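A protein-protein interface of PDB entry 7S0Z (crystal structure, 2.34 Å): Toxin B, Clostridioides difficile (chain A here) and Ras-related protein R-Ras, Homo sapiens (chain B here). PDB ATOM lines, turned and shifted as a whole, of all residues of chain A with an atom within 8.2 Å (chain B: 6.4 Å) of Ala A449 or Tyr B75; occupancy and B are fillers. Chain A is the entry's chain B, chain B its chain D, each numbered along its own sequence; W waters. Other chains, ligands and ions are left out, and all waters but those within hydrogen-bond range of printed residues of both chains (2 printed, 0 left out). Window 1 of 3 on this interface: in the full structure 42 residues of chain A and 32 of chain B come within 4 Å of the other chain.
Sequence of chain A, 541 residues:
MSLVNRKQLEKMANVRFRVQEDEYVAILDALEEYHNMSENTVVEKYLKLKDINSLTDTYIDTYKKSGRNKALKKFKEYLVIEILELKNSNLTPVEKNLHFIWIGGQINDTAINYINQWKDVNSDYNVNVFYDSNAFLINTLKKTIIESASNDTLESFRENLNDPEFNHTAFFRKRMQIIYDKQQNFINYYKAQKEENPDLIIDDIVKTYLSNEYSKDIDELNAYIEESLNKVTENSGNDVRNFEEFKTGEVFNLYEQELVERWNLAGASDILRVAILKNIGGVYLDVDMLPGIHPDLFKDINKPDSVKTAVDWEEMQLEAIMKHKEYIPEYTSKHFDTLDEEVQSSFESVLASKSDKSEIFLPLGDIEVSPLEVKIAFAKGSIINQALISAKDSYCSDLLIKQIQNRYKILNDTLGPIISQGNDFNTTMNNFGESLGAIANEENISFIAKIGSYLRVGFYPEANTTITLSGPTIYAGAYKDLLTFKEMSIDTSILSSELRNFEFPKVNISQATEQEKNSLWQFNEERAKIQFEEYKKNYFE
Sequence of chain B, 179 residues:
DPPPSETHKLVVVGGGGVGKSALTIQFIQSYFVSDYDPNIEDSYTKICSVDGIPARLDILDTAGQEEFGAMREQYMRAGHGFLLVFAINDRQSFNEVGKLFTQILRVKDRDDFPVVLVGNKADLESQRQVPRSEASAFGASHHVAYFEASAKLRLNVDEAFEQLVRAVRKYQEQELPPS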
ATOM      1  N   LEU A 436      -3.004  -3.218  -6.354  1.00  0.00           N
ATOM      2  CA  LEU A 436      -3.658  -4.255  -5.514  1.00  0.00           C
ATOM      3  C   LEU A 436      -5.172  -4.163  -5.694  1.00  0.00           C
ATOM      4  O   LEU A 436      -5.803  -5.222  -5.885  1.00  0.00           O
ATOM      5  CB  LEU A 436      -3.256  -4.085  -4.048  1.00  0.00           C
ATOM      6  CG  LEU A 436      -1.852  -4.587  -3.712  1.00  0.00           C
ATOM      7  CD1 LEU A 436      -1.383  -4.070  -2.361  1.00  0.00           C
ATOM      8  CD2 LEU A 436      -1.787  -6.105  -3.747  1.00  0.00           C
ATOM      9  N   GLY A 437      -5.725  -2.948  -5.658  1.00  0.00           N
ATOM     10  CA  GLY A 437      -7.169  -2.732  -5.873  1.00  0.00           C
ATOM     11  C   GLY A 437      -7.625  -3.313  -7.197  1.00  0.00           C
ATOM     12  O   GLY A 437      -8.758  -3.841  -7.257  1.00  0.00           O
ATOM     13  N   ALA A 440      -8.085  -7.156  -6.894  1.00  0.00           N
ATOM     14  CA  ALA A 440      -8.839  -7.641  -5.718  1.00  0.00           C
ATOM     15  C   ALA A 440     -10.169  -8.231  -6.176  1.00  0.00           C
ATOM     16  O   ALA A 440     -10.790  -7.692  -7.105  1.00  0.00           O
ATOM     17  CB  ALA A 440      -9.057  -6.549  -4.707  1.00  0.00           C
ATOM     18  N   ASN A 444      -9.958 -12.942  -2.444  1.00  0.00           N
ATOM     19  CA  ASN A 444      -8.562 -12.640  -2.019  1.00  0.00           C
ATOM     20  C   ASN A 444      -8.440 -11.298  -1.283  1.00  0.00           C
ATOM     21  O   ASN A 444      -7.309 -10.968  -0.891  1.00  0.00           O
ATOM     22  CB  ASN A 444      -7.596 -12.680  -3.205  1.00  0.00           C
ATOM     23  CG  ASN A 444      -7.793 -11.553  -4.197  1.00  0.00           C
ATOM     24  OD1 ASN A 444      -8.414 -10.536  -3.892  1.00  0.00           O
ATOM     25  ND2 ASN A 444      -7.244 -11.718  -5.387  1.00  0.00           N
ATOM     26  N   ILE A 445      -9.527 -10.551  -1.088  1.00  0.00           N
ATOM     27  CA  ILE A 445      -9.423  -9.132  -0.627  1.00  0.00           C
ATOM     28  C   ILE A 445      -8.756  -9.066   0.756  1.00  0.00           C
ATOM     29  O   ILE A 445      -7.991  -8.109   0.978  1.00  0.00           O
ATOM     30  CB  ILE A 445     -10.780  -8.398  -0.665  1.00  0.00           C
ATOM     31  CG1 ILE A 445     -10.656  -6.972  -0.122  1.00  0.00           C
ATOM     32  CG2 ILE A 445     -11.872  -9.158   0.076  1.00  0.00           C
ATOM     33  CD1 ILE A 445      -9.681  -6.094  -0.866  1.00  0.00           C
ATOM     34  N   SER A 446      -9.017 -10.021   1.649  1.00  0.00           N
ATOM     35  CA  SER A 446      -8.382 -10.070   2.997  1.00  0.00           C
ATOM     36  C   SER A 446      -6.860 -10.140   2.845  1.00  0.00           C
ATOM     37  O   SER A 446      -6.151  -9.300   3.430  1.00  0.00           O
ATOM     38  CB  SER A 446      -8.880 -11.233   3.819  1.00  0.00           C
ATOM     39  OG  SER A 446     -10.080 -10.906   4.495  1.00  0.00           O
ATOM     40  N   PHE A 447      -6.381 -11.127   2.098  1.00  0.00           N
ATOM     41  CA  PHE A 447      -4.950 -11.252   1.735  1.00  0.00           C
ATOM     42  C   PHE A 447      -4.446  -9.933   1.147  1.00  0.00           C
ATOM     43  O   PHE A 447      -3.420  -9.407   1.626  1.00  0.00           O
ATOM     44  CB  PHE A 447      -4.779 -12.390   0.737  1.00  0.00           C
ATOM     45  CG  PHE A 447      -3.379 -12.522   0.219  1.00  0.00           C
ATOM     46  CD1 PHE A 447      -2.419 -13.170   0.975  1.00  0.00           C
ATOM     47  CD2 PHE A 447      -3.025 -11.991  -1.010  1.00  0.00           C
ATOM     48  CE1 PHE A 447      -1.124 -13.292   0.506  1.00  0.00           C
ATOM     49  CE2 PHE A 447      -1.728 -12.117  -1.481  1.00  0.00           C
ATOM     50  CZ  PHE A 447      -0.782 -12.770  -0.722  1.00  0.00           C
ATOM     51  N   ILE A 448      -5.149  -9.407   0.145  1.00  0.00           N
ATOM     52  CA  ILE A 448      -4.708  -8.189  -0.596  1.00  0.00           C
ATOM     53  C   ILE A 448      -4.541  -7.034   0.388  1.00  0.00           C
ATOM     54  O   ILE A 448      -3.527  -6.322   0.292  1.00  0.00           O
ATOM     55  CB  ILE A 448      -5.683  -7.847  -1.733  1.00  0.00           C
ATOM     56  CG1 ILE A 448      -5.596  -8.893  -2.842  1.00  0.00           C
ATOM     57  CG2 ILE A 448      -5.407  -6.456  -2.276  1.00  0.00           C
ATOM     58  CD1 ILE A 448      -4.266  -8.885  -3.554  1.00  0.00           C
ATOM     59  N   ALA A 449      -5.485  -6.861   1.308  1.00  0.00           N
ATOM     60  CA  ALA A 449      -5.409  -5.784   2.318  1.00  0.00           C
ATOM     61  C   ALA A 449      -4.216  -6.010   3.253  1.00  0.00           C
ATOM     62  O   ALA A 449      -3.707  -5.007   3.790  1.00  0.00           O
ATOM     63  CB  ALA A 449      -6.704  -5.683   3.081  1.00  0.00           C
ATOM     64  N   LYS A 450      -3.768  -7.252   3.451  1.00  0.00           N
ATOM     65  CA  LYS A 450      -2.725  -7.526   4.471  1.00  0.00           C
ATOM     66  C   LYS A 450      -1.313  -7.454   3.888  1.00  0.00           C
ATOM     67  O   LYS A 450      -0.368  -7.469   4.696  1.00  0.00           O
ATOM     68  CB  LYS A 450      -2.977  -8.872   5.142  1.00  0.00           C
ATOM     69  CG  LYS A 450      -4.247  -8.882   5.972  1.00  0.00           C
ATOM     70  CD  LYS A 450      -4.701 -10.252   6.380  1.00  0.00           C
ATOM     71  CE  LYS A 450      -5.323 -10.230   7.760  1.00  0.00           C
ATOM     72  NZ  LYS A 450      -5.850 -11.557   8.157  1.00  0.00           N
ATOM     73  N   ILE A 451      -1.147  -7.357   2.569  1.00  0.00           N
ATOM     74  CA  ILE A 451       0.229  -7.353   1.986  1.00  0.00           C
ATOM     75  C   ILE A 451       0.645  -5.942   1.566  1.00  0.00           C
ATOM     76  O   ILE A 451       1.775  -5.815   1.068  1.00  0.00           O
ATOM     77  CB  ILE A 451       0.365  -8.340   0.819  1.00  0.00           C
ATOM     78  CG1 ILE A 451      -0.344  -7.843  -0.439  1.00  0.00           C
ATOM     79  CG2 ILE A 451      -0.094  -9.729   1.238  1.00  0.00           C
ATOM     80  CD1 ILE A 451      -0.076  -8.708  -1.640  1.00  0.00           C
ATOM     81  N   GLY A 452      -0.190  -4.925   1.778  1.00  0.00           N
ATOM     82  CA  GLY A 452       0.161  -3.538   1.405  1.00  0.00           C
ATOM     83  C   GLY A 452       1.318  -2.990   2.228  1.00  0.00           C
ATOM     84  O   GLY A 452       1.987  -2.051   1.750  1.00  0.00           O
ATOM     85  N   SER A 453       1.568  -3.555   3.413  1.00  0.00           N
ATOM     86  CA  SER A 453       2.612  -3.071   4.354  1.00  0.00           C
ATOM     87  C   SER A 453       3.934  -3.811   4.162  1.00  0.00           C
ATOM     88  O   SER A 453       4.780  -3.735   5.069  1.00  0.00           O
ATOM     89  CB  SER A 453       2.143  -3.195   5.768  1.00  0.00           C
ATOM     90  OG  SER A 453       1.222  -2.163   6.066  1.00  0.00           O
ATOM     91  N   TYR A 454       4.125  -4.482   3.032  1.00  0.00           N
ATOM     92  CA  TYR A 454       5.285  -5.382   2.827  1.00  0.00           C
ATOM     93  C   TYR A 454       6.590  -4.602   2.990  1.00  0.00           C
ATOM     94  O   TYR A 454       7.471  -5.062   3.740  1.00  0.00           O
ATOM     95  CB  TYR A 454       5.217  -6.044   1.456  1.00  0.00           C
ATOM     96  CG  TYR A 454       6.329  -7.026   1.198  1.00  0.00           C
ATOM     97  CD1 TYR A 454       6.476  -8.159   1.982  1.00  0.00           C
ATOM     98  CD2 TYR A 454       7.236  -6.822   0.172  1.00  0.00           C
ATOM     99  CE1 TYR A 454       7.488  -9.074   1.746  1.00  0.00           C
ATOM    100  CE2 TYR A 454       8.253  -7.727  -0.078  1.00  0.00           C
ATOM    101  CZ  TYR A 454       8.377  -8.858   0.710  1.00  0.00           C
ATOM    102  OH  TYR A 454       9.380  -9.750   0.470  1.00  0.00           O
ATOM    103  N   ARG A 456       7.228  -2.045   4.579  1.00  0.00           N
ATOM    104  CA  ARG A 456       7.410  -1.468   5.931  1.00  0.00           C
ATOM    105  C   ARG A 456       7.926  -2.515   6.920  1.00  0.00           C
ATOM    106  O   ARG A 456       8.272  -2.118   8.048  1.00  0.00           O
ATOM    107  CB  ARG A 456       6.089  -0.919   6.463  1.00  0.00           C
ATOM    108  CG  ARG A 456       5.477   0.185   5.621  1.00  0.00           C
ATOM    109  CD  ARG A 456       4.207   0.624   6.313  1.00  0.00           C
ATOM    110  NE  ARG A 456       3.543   1.733   5.655  1.00  0.00           N
ATOM    111  CZ  ARG A 456       2.252   1.783   5.359  1.00  0.00           C
ATOM    112  NH1 ARG A 456       1.449   0.771   5.650  1.00  0.00           N
ATOM    113  NH2 ARG A 456       1.766   2.858   4.770  1.00  0.00           N
ATOM    114  N   GLU A 462       3.151  -2.052  13.527  1.00  0.00           N
ATOM    115  CA  GLU A 462       2.063  -2.939  13.031  1.00  0.00           C
ATOM    116  C   GLU A 462       2.239  -3.286  11.549  1.00  0.00           C
ATOM    117  O   GLU A 462       1.203  -3.410  10.864  1.00  0.00           O
ATOM    118  CB  GLU A 462       0.679  -2.306  13.206  1.00  0.00           C
ATOM    119  CG  GLU A 462       0.528  -1.466  14.459  1.00  0.00           C
ATOM    120  CD  GLU A 462      -0.101  -2.173  15.650  1.00  0.00           C
ATOM    121  OE1 GLU A 462      -0.327  -3.401  15.566  1.00  0.00           O
ATOM    122  OE2 GLU A 462      -0.368  -1.490  16.664  1.00  0.00           O
ATOM    123  N   ASN A 464       2.590  -6.250   9.760  1.00  0.00           N
ATOM    124  CA  ASN A 464       2.453  -7.686  10.115  1.00  0.00           C
ATOM    125  C   ASN A 464       2.387  -8.577   8.876  1.00  0.00           C
ATOM    126  O   ASN A 464       2.013  -9.753   9.038  1.00  0.00           O
ATOM    127  CB  ASN A 464       1.199  -7.940  10.947  1.00  0.00           C
ATOM    128  CG  ASN A 464       1.102  -7.013  12.133  1.00  0.00           C
ATOM    129  OD1 ASN A 464       0.031  -6.487  12.424  1.00  0.00           O
ATOM    130  ND2 ASN A 464       2.214  -6.804  12.819  1.00  0.00           N
ATOM    131  N   THR A 465       2.769  -8.070   7.707  1.00  0.00           N
ATOM    132  CA  THR A 465       2.604  -8.787   6.413  1.00  0.00           C
ATOM    133  C   THR A 465       3.200 -10.200   6.477  1.00  0.00           C
ATOM    134  O   THR A 465       2.642 -11.085   5.804  1.00  0.00           O
ATOM    135  CB  THR A 465       3.184  -7.969   5.258  1.00  0.00           C
ATOM    136  OG1 THR A 465       2.348  -6.820   5.119  1.00  0.00           O
ATOM    137  CG2 THR A 465       3.209  -8.723   3.948  1.00  0.00           C
ATOM    138  N   THR A 468       1.027 -13.173   6.976  1.00  0.00           N
ATOM    139  CA  THR A 468       0.159 -13.452   5.813  1.00  0.00           C
ATOM    140  C   THR A 468       0.949 -14.172   4.716  1.00  0.00           C
ATOM    141  O   THR A 468       0.381 -15.097   4.109  1.00  0.00           O
ATOM    142  CB  THR A 468      -0.465 -12.155   5.301  1.00  0.00           C
ATOM    143  OG1 THR A 468      -1.377 -11.662   6.282  1.00  0.00           O
ATOM    144  CG2 THR A 468      -1.196 -12.362   3.999  1.00  0.00           C
ATOM    145  N   VAL B  11     -15.155  -5.758   9.306  1.00  0.00           N
ATOM    146  CA  VAL B  11     -13.827  -5.121   9.435  1.00  0.00           C
ATOM    147  C   VAL B  11     -13.827  -4.305  10.718  1.00  0.00           C
ATOM    148  O   VAL B  11     -14.731  -3.475  10.907  1.00  0.00           O
ATOM    149  CB  VAL B  11     -13.496  -4.288   8.193  1.00  0.00           C
ATOM    150  CG1 VAL B  11     -12.228  -3.476   8.399  1.00  0.00           C
ATOM    151  CG2 VAL B  11     -13.384  -5.197   6.980  1.00  0.00           C
ATOM    152  N   VAL B  13     -11.974  -1.506  12.656  1.00  0.00           N
ATOM    153  CA  VAL B  13     -11.108  -0.342  12.318  1.00  0.00           C
ATOM    154  C   VAL B  13     -10.995   0.567  13.531  1.00  0.00           C
ATOM    155  O   VAL B  13     -11.896   0.551  14.395  1.00  0.00           O
ATOM    156  CB  VAL B  13     -11.640   0.452  11.115  1.00  0.00           C
ATOM    157  CG1 VAL B  13     -11.232  -0.201   9.814  1.00  0.00           C
ATOM    158  CG2 VAL B  13     -13.148   0.649  11.193  1.00  0.00           C
ATOM    159  N   LEU B  60     -11.886  -9.072   9.910  1.00  0.00           N
ATOM    160  CA  LEU B  60     -10.599  -8.519   9.453  1.00  0.00           C
ATOM    161  C   LEU B  60     -10.291  -7.290  10.299  1.00  0.00           C
ATOM    162  O   LEU B  60     -11.060  -6.316  10.236  1.00  0.00           O
ATOM    163  CB  LEU B  60     -10.708  -8.160   7.976  1.00  0.00           C
ATOM    164  CG  LEU B  60      -9.487  -7.447   7.408  1.00  0.00           C
ATOM    165  CD1 LEU B  60      -8.296  -8.392   7.360  1.00  0.00           C
ATOM    166  CD2 LEU B  60      -9.801  -6.881   6.035  1.00  0.00           C
ATOM    167  N   ASP B  61      -9.205  -7.361  11.062  1.00  0.00           N
ATOM    168  CA  ASP B  61      -8.709  -6.222  11.868  1.00  0.00           C
ATOM    169  C   ASP B  61      -7.742  -5.418  11.016  1.00  0.00           C
ATOM    170  O   ASP B  61      -6.880  -6.032  10.360  1.00  0.00           O
ATOM    171  CB  ASP B  61      -7.928  -6.681  13.092  1.00  0.00           C
ATOM    172  CG  ASP B  61      -8.776  -7.404  14.114  1.00  0.00           C
ATOM    173  OD1 ASP B  61     -10.014  -7.349  13.997  1.00  0.00           O
ATOM    174  OD2 ASP B  61      -8.188  -8.021  15.015  1.00  0.00           O
ATOM    175  N   THR B  62      -7.839  -4.097  11.068  1.00  0.00           N
ATOM    176  CA  THR B  62      -6.873  -3.226  10.359  1.00  0.00           C
ATOM    177  C   THR B  62      -5.605  -3.108  11.201  1.00  0.00           C
ATOM    178  O   THR B  62      -5.602  -3.611  12.345  1.00  0.00           O
ATOM    179  CB  THR B  62      -7.467  -1.855  10.044  1.00  0.00           C
ATOM    180  OG1 THR B  62      -8.083  -1.340  11.223  1.00  0.00           O
ATOM    181  CG2 THR B  62      -8.474  -1.918   8.923  1.00  0.00           C
ATOM    182  N   ALA B  63      -4.577  -2.441  10.673  1.00  0.00           N
ATOM    183  CA  ALA B  63      -3.237  -2.435  11.329  1.00  0.00           C
ATOM    184  C   ALA B  63      -2.988  -1.218  12.245  1.00  0.00           C
ATOM    185  O   ALA B  63      -2.722  -1.401  13.476  1.00  0.00           O
ATOM    186  CB  ALA B  63      -2.162  -2.480  10.287  1.00  0.00           C
ATOM    187  N   GLU B  66      -3.478   4.035   8.696  1.00  0.00           N
ATOM    188  CA  GLU B  66      -2.872   3.809   7.365  1.00  0.00           C
ATOM    189  C   GLU B  66      -2.831   5.150   6.637  1.00  0.00           C
ATOM    190  O   GLU B  66      -3.885   5.795   6.515  1.00  0.00           O
ATOM    191  CB  GLU B  66      -3.651   2.759   6.581  1.00  0.00           C
ATOM    192  CG  GLU B  66      -3.176   2.612   5.152  1.00  0.00           C
ATOM    193  CD  GLU B  66      -1.721   2.195   5.040  1.00  0.00           C
ATOM    194  OE1 GLU B  66      -1.397   1.077   5.473  1.00  0.00           O
ATOM    195  OE2 GLU B  66      -0.913   3.000   4.539  1.00  0.00           O
ATOM    196  N   ALA B  70      -5.005   4.423  -1.010  1.00  0.00           N
ATOM    197  CA  ALA B  70      -5.142   3.179  -1.801  1.00  0.00           C
ATOM    198  C   ALA B  70      -5.155   1.965  -0.866  1.00  0.00           C
ATOM    199  O   ALA B  70      -5.954   1.040  -1.126  1.00  0.00           O
ATOM    200  CB  ALA B  70      -4.045   3.072  -2.824  1.00  0.00           C
ATOM    201  N   MET B  71      -4.331   1.967   0.186  1.00  0.00           N
ATOM    202  CA  MET B  71      -4.249   0.818   1.126  1.00  0.00           C
ATOM    203  C   MET B  71      -5.463   0.805   2.051  1.00  0.00           C
ATOM    204  O   MET B  71      -6.020  -0.285   2.273  1.00  0.00           O
ATOM    205  CB  MET B  71      -2.976   0.856   1.969  1.00  0.00           C
ATOM    206  CG  MET B  71      -1.933  -0.092   1.447  1.00  0.00           C
ATOM    207  SD  MET B  71      -1.262   0.561  -0.086  1.00  0.00           S
ATOM    208  CE  MET B  71       0.251  -0.381  -0.250  1.00  0.00           C
ATOM    209  N   ARG B  72      -5.831   1.961   2.592  1.00  0.00           N
ATOM    210  CA  ARG B  72      -7.012   2.078   3.485  1.00  0.00           C
ATOM    211  C   ARG B  72      -8.261   1.624   2.726  1.00  0.00           C
ATOM    212  O   ARG B  72      -9.132   0.988   3.348  1.00  0.00           O
ATOM    213  CB  ARG B  72      -7.160   3.521   3.965  1.00  0.00           C
ATOM    214  CG  ARG B  72      -7.362   3.646   5.466  1.00  0.00           C
ATOM    215  CD  ARG B  72      -6.999   5.035   5.945  1.00  0.00           C
ATOM    216  NE  ARG B  72      -7.336   6.065   4.964  1.00  0.00           N
ATOM    217  CZ  ARG B  72      -6.473   6.907   4.393  1.00  0.00           C
ATOM    218  NH1 ARG B  72      -5.188   6.879   4.708  1.00  0.00           N
ATOM    219  NH2 ARG B  72      -6.905   7.792   3.512  1.00  0.00           N
ATOM    220  N   GLU B  73      -8.323   1.919   1.428  1.00  0.00           N
ATOM    221  CA  GLU B  73      -9.479   1.573   0.561  1.00  0.00           C
ATOM    222  C   GLU B  73      -9.675   0.056   0.499  1.00  0.00           C
ATOM    223  O   GLU B  73     -10.844  -0.381   0.480  1.00  0.00           O
ATOM    224  CB  GLU B  73      -9.262   2.142  -0.837  1.00  0.00           C
ATOM    225  CG  GLU B  73     -10.415   1.890  -1.786  1.00  0.00           C
ATOM    226  CD  GLU B  73     -10.914   3.146  -2.480  1.00  0.00           C
ATOM    227  OE1 GLU B  73     -10.220   4.184  -2.408  1.00  0.00           O
ATOM    228  OE2 GLU B  73     -12.005   3.087  -3.083  1.00  0.00           O
ATOM    229  N   GLN B  74      -8.594  -0.721   0.451  1.00  0.00           N
ATOM    230  CA  GLN B  74      -8.713  -2.195   0.303  1.00  0.00           C
ATOM    231  C   GLN B  74      -9.381  -2.769   1.556  1.00  0.00           C
ATOM    232  O   GLN B  74     -10.214  -3.682   1.411  1.00  0.00           O
ATOM    233  CB  GLN B  74      -7.356  -2.841   0.028  1.00  0.00           C
ATOM    234  CG  GLN B  74      -6.659  -2.306  -1.221  1.00  0.00           C
ATOM    235  CD  GLN B  74      -7.560  -2.179  -2.428  1.00  0.00           C
ATOM    236  OE1 GLN B  74      -8.284  -3.103  -2.787  1.00  0.00           O
ATOM    237  NE2 GLN B  74      -7.517  -1.024  -3.073  1.00  0.00           N
ATOM    238  N   TYR B  75      -9.067  -2.231   2.732  1.00  0.00           N
ATOM    239  CA  TYR B  75      -9.708  -2.661   4.001  1.00  0.00           C
ATOM    240  C   TYR B  75     -11.212  -2.401   3.953  1.00  0.00           C
ATOM    241  O   TYR B  75     -11.965  -3.177   4.571  1.00  0.00           O
ATOM    242  CB  TYR B  75      -9.070  -1.972   5.206  1.00  0.00           C
ATOM    243  CG  TYR B  75      -7.869  -2.717   5.722  1.00  0.00           C
ATOM    244  CD1 TYR B  75      -8.018  -3.964   6.305  1.00  0.00           C
ATOM    245  CD2 TYR B  75      -6.585  -2.210   5.599  1.00  0.00           C
ATOM    246  CE1 TYR B  75      -6.929  -4.677   6.782  1.00  0.00           C
ATOM    247  CE2 TYR B  75      -5.483  -2.912   6.068  1.00  0.00           C
ATOM    248  CZ  TYR B  75      -5.655  -4.152   6.661  1.00  0.00           C
ATOM    249  OH  TYR B  75      -4.588  -4.863   7.129  1.00  0.00           O
ATOM    250  N   MET B  76     -11.637  -1.358   3.243  1.00  0.00           N
ATOM    251  CA  MET B  76     -13.053  -0.912   3.278  1.00  0.00           C
ATOM    252  C   MET B  76     -13.863  -1.629   2.205  1.00  0.00           C
ATOM    253  O   MET B  76     -15.041  -1.904   2.458  1.00  0.00           O
ATOM    254  CB  MET B  76     -13.153   0.600   3.099  1.00  0.00           C
ATOM    255  CG  MET B  76     -12.232   1.309   4.043  1.00  0.00           C
ATOM    256  SD  MET B  76     -12.638   3.031   4.297  1.00  0.00           S
ATOM    257  CE  MET B  76     -12.192   3.151   6.026  1.00  0.00           C
ATOM    258  N   ARG B  77     -13.254  -1.942   1.067  1.00  0.00           N
ATOM    259  CA  ARG B  77     -13.905  -2.832   0.077  1.00  0.00           C
ATOM    260  C   ARG B  77     -14.268  -4.153   0.765  1.00  0.00           C
ATOM    261  O   ARG B  77     -15.345  -4.694   0.453  1.00  0.00           O
ATOM    262  CB  ARG B  77     -12.991  -3.024  -1.130  1.00  0.00           C
ATOM    263  CG  ARG B  77     -12.825  -1.749  -1.944  1.00  0.00           C
ATOM    264  CD  ARG B  77     -11.888  -1.925  -3.119  1.00  0.00           C
ATOM    265  NE  ARG B  77     -12.363  -2.948  -4.042  1.00  0.00           N
ATOM    266  CZ  ARG B  77     -11.662  -3.427  -5.064  1.00  0.00           C
ATOM    267  NH1 ARG B  77     -10.442  -2.974  -5.305  1.00  0.00           N
ATOM    268  NH2 ARG B  77     -12.181  -4.359  -5.844  1.00  0.00           N
ATOM    269  N   ALA B  78     -13.439  -4.628   1.700  1.00  0.00           N
ATOM    270  CA  ALA B  78     -13.587  -5.978   2.296  1.00  0.00           C
ATOM    271  C   ALA B  78     -14.785  -6.049   3.248  1.00  0.00           C
ATOM    272  O   ALA B  78     -15.235  -7.173   3.511  1.00  0.00           O
ATOM    273  CB  ALA B  78     -12.330  -6.388   3.017  1.00  0.00           C
ATOM    274  N   GLY B  79     -15.276  -4.919   3.756  1.00  0.00           N
ATOM    275  CA  GLY B  79     -16.252  -4.918   4.860  1.00  0.00           C
ATOM    276  C   GLY B  79     -17.676  -4.812   4.362  1.00  0.00           C
ATOM    277  O   GLY B  79     -17.974  -3.858   3.624  1.00  0.00           O
ATOM    278  N   PHE B  82     -18.726  -2.559   9.686  1.00  0.00           N
ATOM    279  CA  PHE B  82     -17.512  -2.029  10.341  1.00  0.00           C
ATOM    280  C   PHE B  82     -17.749  -1.910  11.835  1.00  0.00           C
ATOM    281  O   PHE B  82     -18.716  -1.250  12.250  1.00  0.00           O
ATOM    282  CB  PHE B  82     -17.127  -0.682   9.736  1.00  0.00           C
ATOM    283  CG  PHE B  82     -16.652  -0.787   8.312  1.00  0.00           C
ATOM    284  CD1 PHE B  82     -15.347  -1.159   8.029  1.00  0.00           C
ATOM    285  CD2 PHE B  82     -17.519  -0.546   7.259  1.00  0.00           C
ATOM    286  CE1 PHE B  82     -14.912  -1.271   6.716  1.00  0.00           C
ATOM    287  CE2 PHE B  82     -17.084  -0.656   5.950  1.00  0.00           C
ATOM    288  CZ  PHE B  82     -15.784  -1.017   5.679  1.00  0.00           C
HETATM  289  O   HOH W   1     -10.784  -5.393  -8.081  1.00  0.00           O
HETATM  290  O   HOH W   2      -4.109  -2.428   2.849  1.00  0.00           O
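The guanidinium group (NH1) of Arg B77 is in hydrogen-bond range of the backbone carbonyl oxygen (O) of Gly A437, at 2.7 Å. OE2 of Glu B66 lies within salt-bridge range of NH2 of Arg A456 (2.7 Å). O of Ala A449 is in hydrogen-bond range of OH of Tyr B75, 3.5 Å away.
Among the printed residues, merely in contact across the chains: Gly A452 with Met B71, Gly A437 with Gln B74, Ile A445 with Gln B74, Glu A462 with Ala B63, Lys A450 with Leu B60, Ile A445 with Ala B78 and Ala A440 with Arg B77.
Hydrophobic or aromatic side chains of chain A within 4 Å of the printed part of chain B: Ala A440, Ile A445 and Ala A449. Of the 18 printed residues of chain B, 8 touch a printed residue of chain A. Hydrophobic or aromatic side chains of chain B that line the printed part of chain A: Leu B60, Ala B63, Met B71, Tyr B75 and Ala B78. Among the printed residues, 10 pairs touch across the chains. Among the printed residues, Asp or Glu carboxylates within 4 Å of a Lys or Arg side-chain nitrogen of the other chain: Arg A456 with Glu B66 (2.7 Å).
Water W1 lies within hydrogen-bond range of O of Ala A440 (2.5 Å), O of Gly A437 (2.7 Å) and NH2 of Arg B77 (2.8 Å). Water W2 lies within hydrogen-bond range of the backbone carbonyl oxygen (O) of Ala A449 and the backbone carbonyl oxygen (O) of Met B71.
Printed residues of chain B within 4 Å of Ala A440: Arg B77. Of the printed residues of chain B, Ile A445 touches Gln B74 and Ala B78. Of chain B, only Tyr B75 (3.5 Å) comes within 4 Å of Ala A449. Printed residues of chain A within 4 Å of Ala B63: Glu A462. Of the printed residues of chain A, Tyr B75 touches Ala A449 (3.5 Å).
O of Glu B66 sits at hydrogen-bond distance from NH1 of Arg B72 (2.5 Å). NE2 of Gln B74 sits at hydrogen-bond distance from O of Ala B70, at 3.2 Å. The backbone carbonyl oxygen (O) of Lys A450 is in hydrogen-bond range of the side-chain hydroxyl (OG1) of Thr A465 (2.8 Å). OG of Ser A453 is in hydrogen-bond range of NH1 of Arg A456, 3.0 Å away. OE1 of Gln B74 is in hydrogen-bond range of NH1 of Arg B77.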
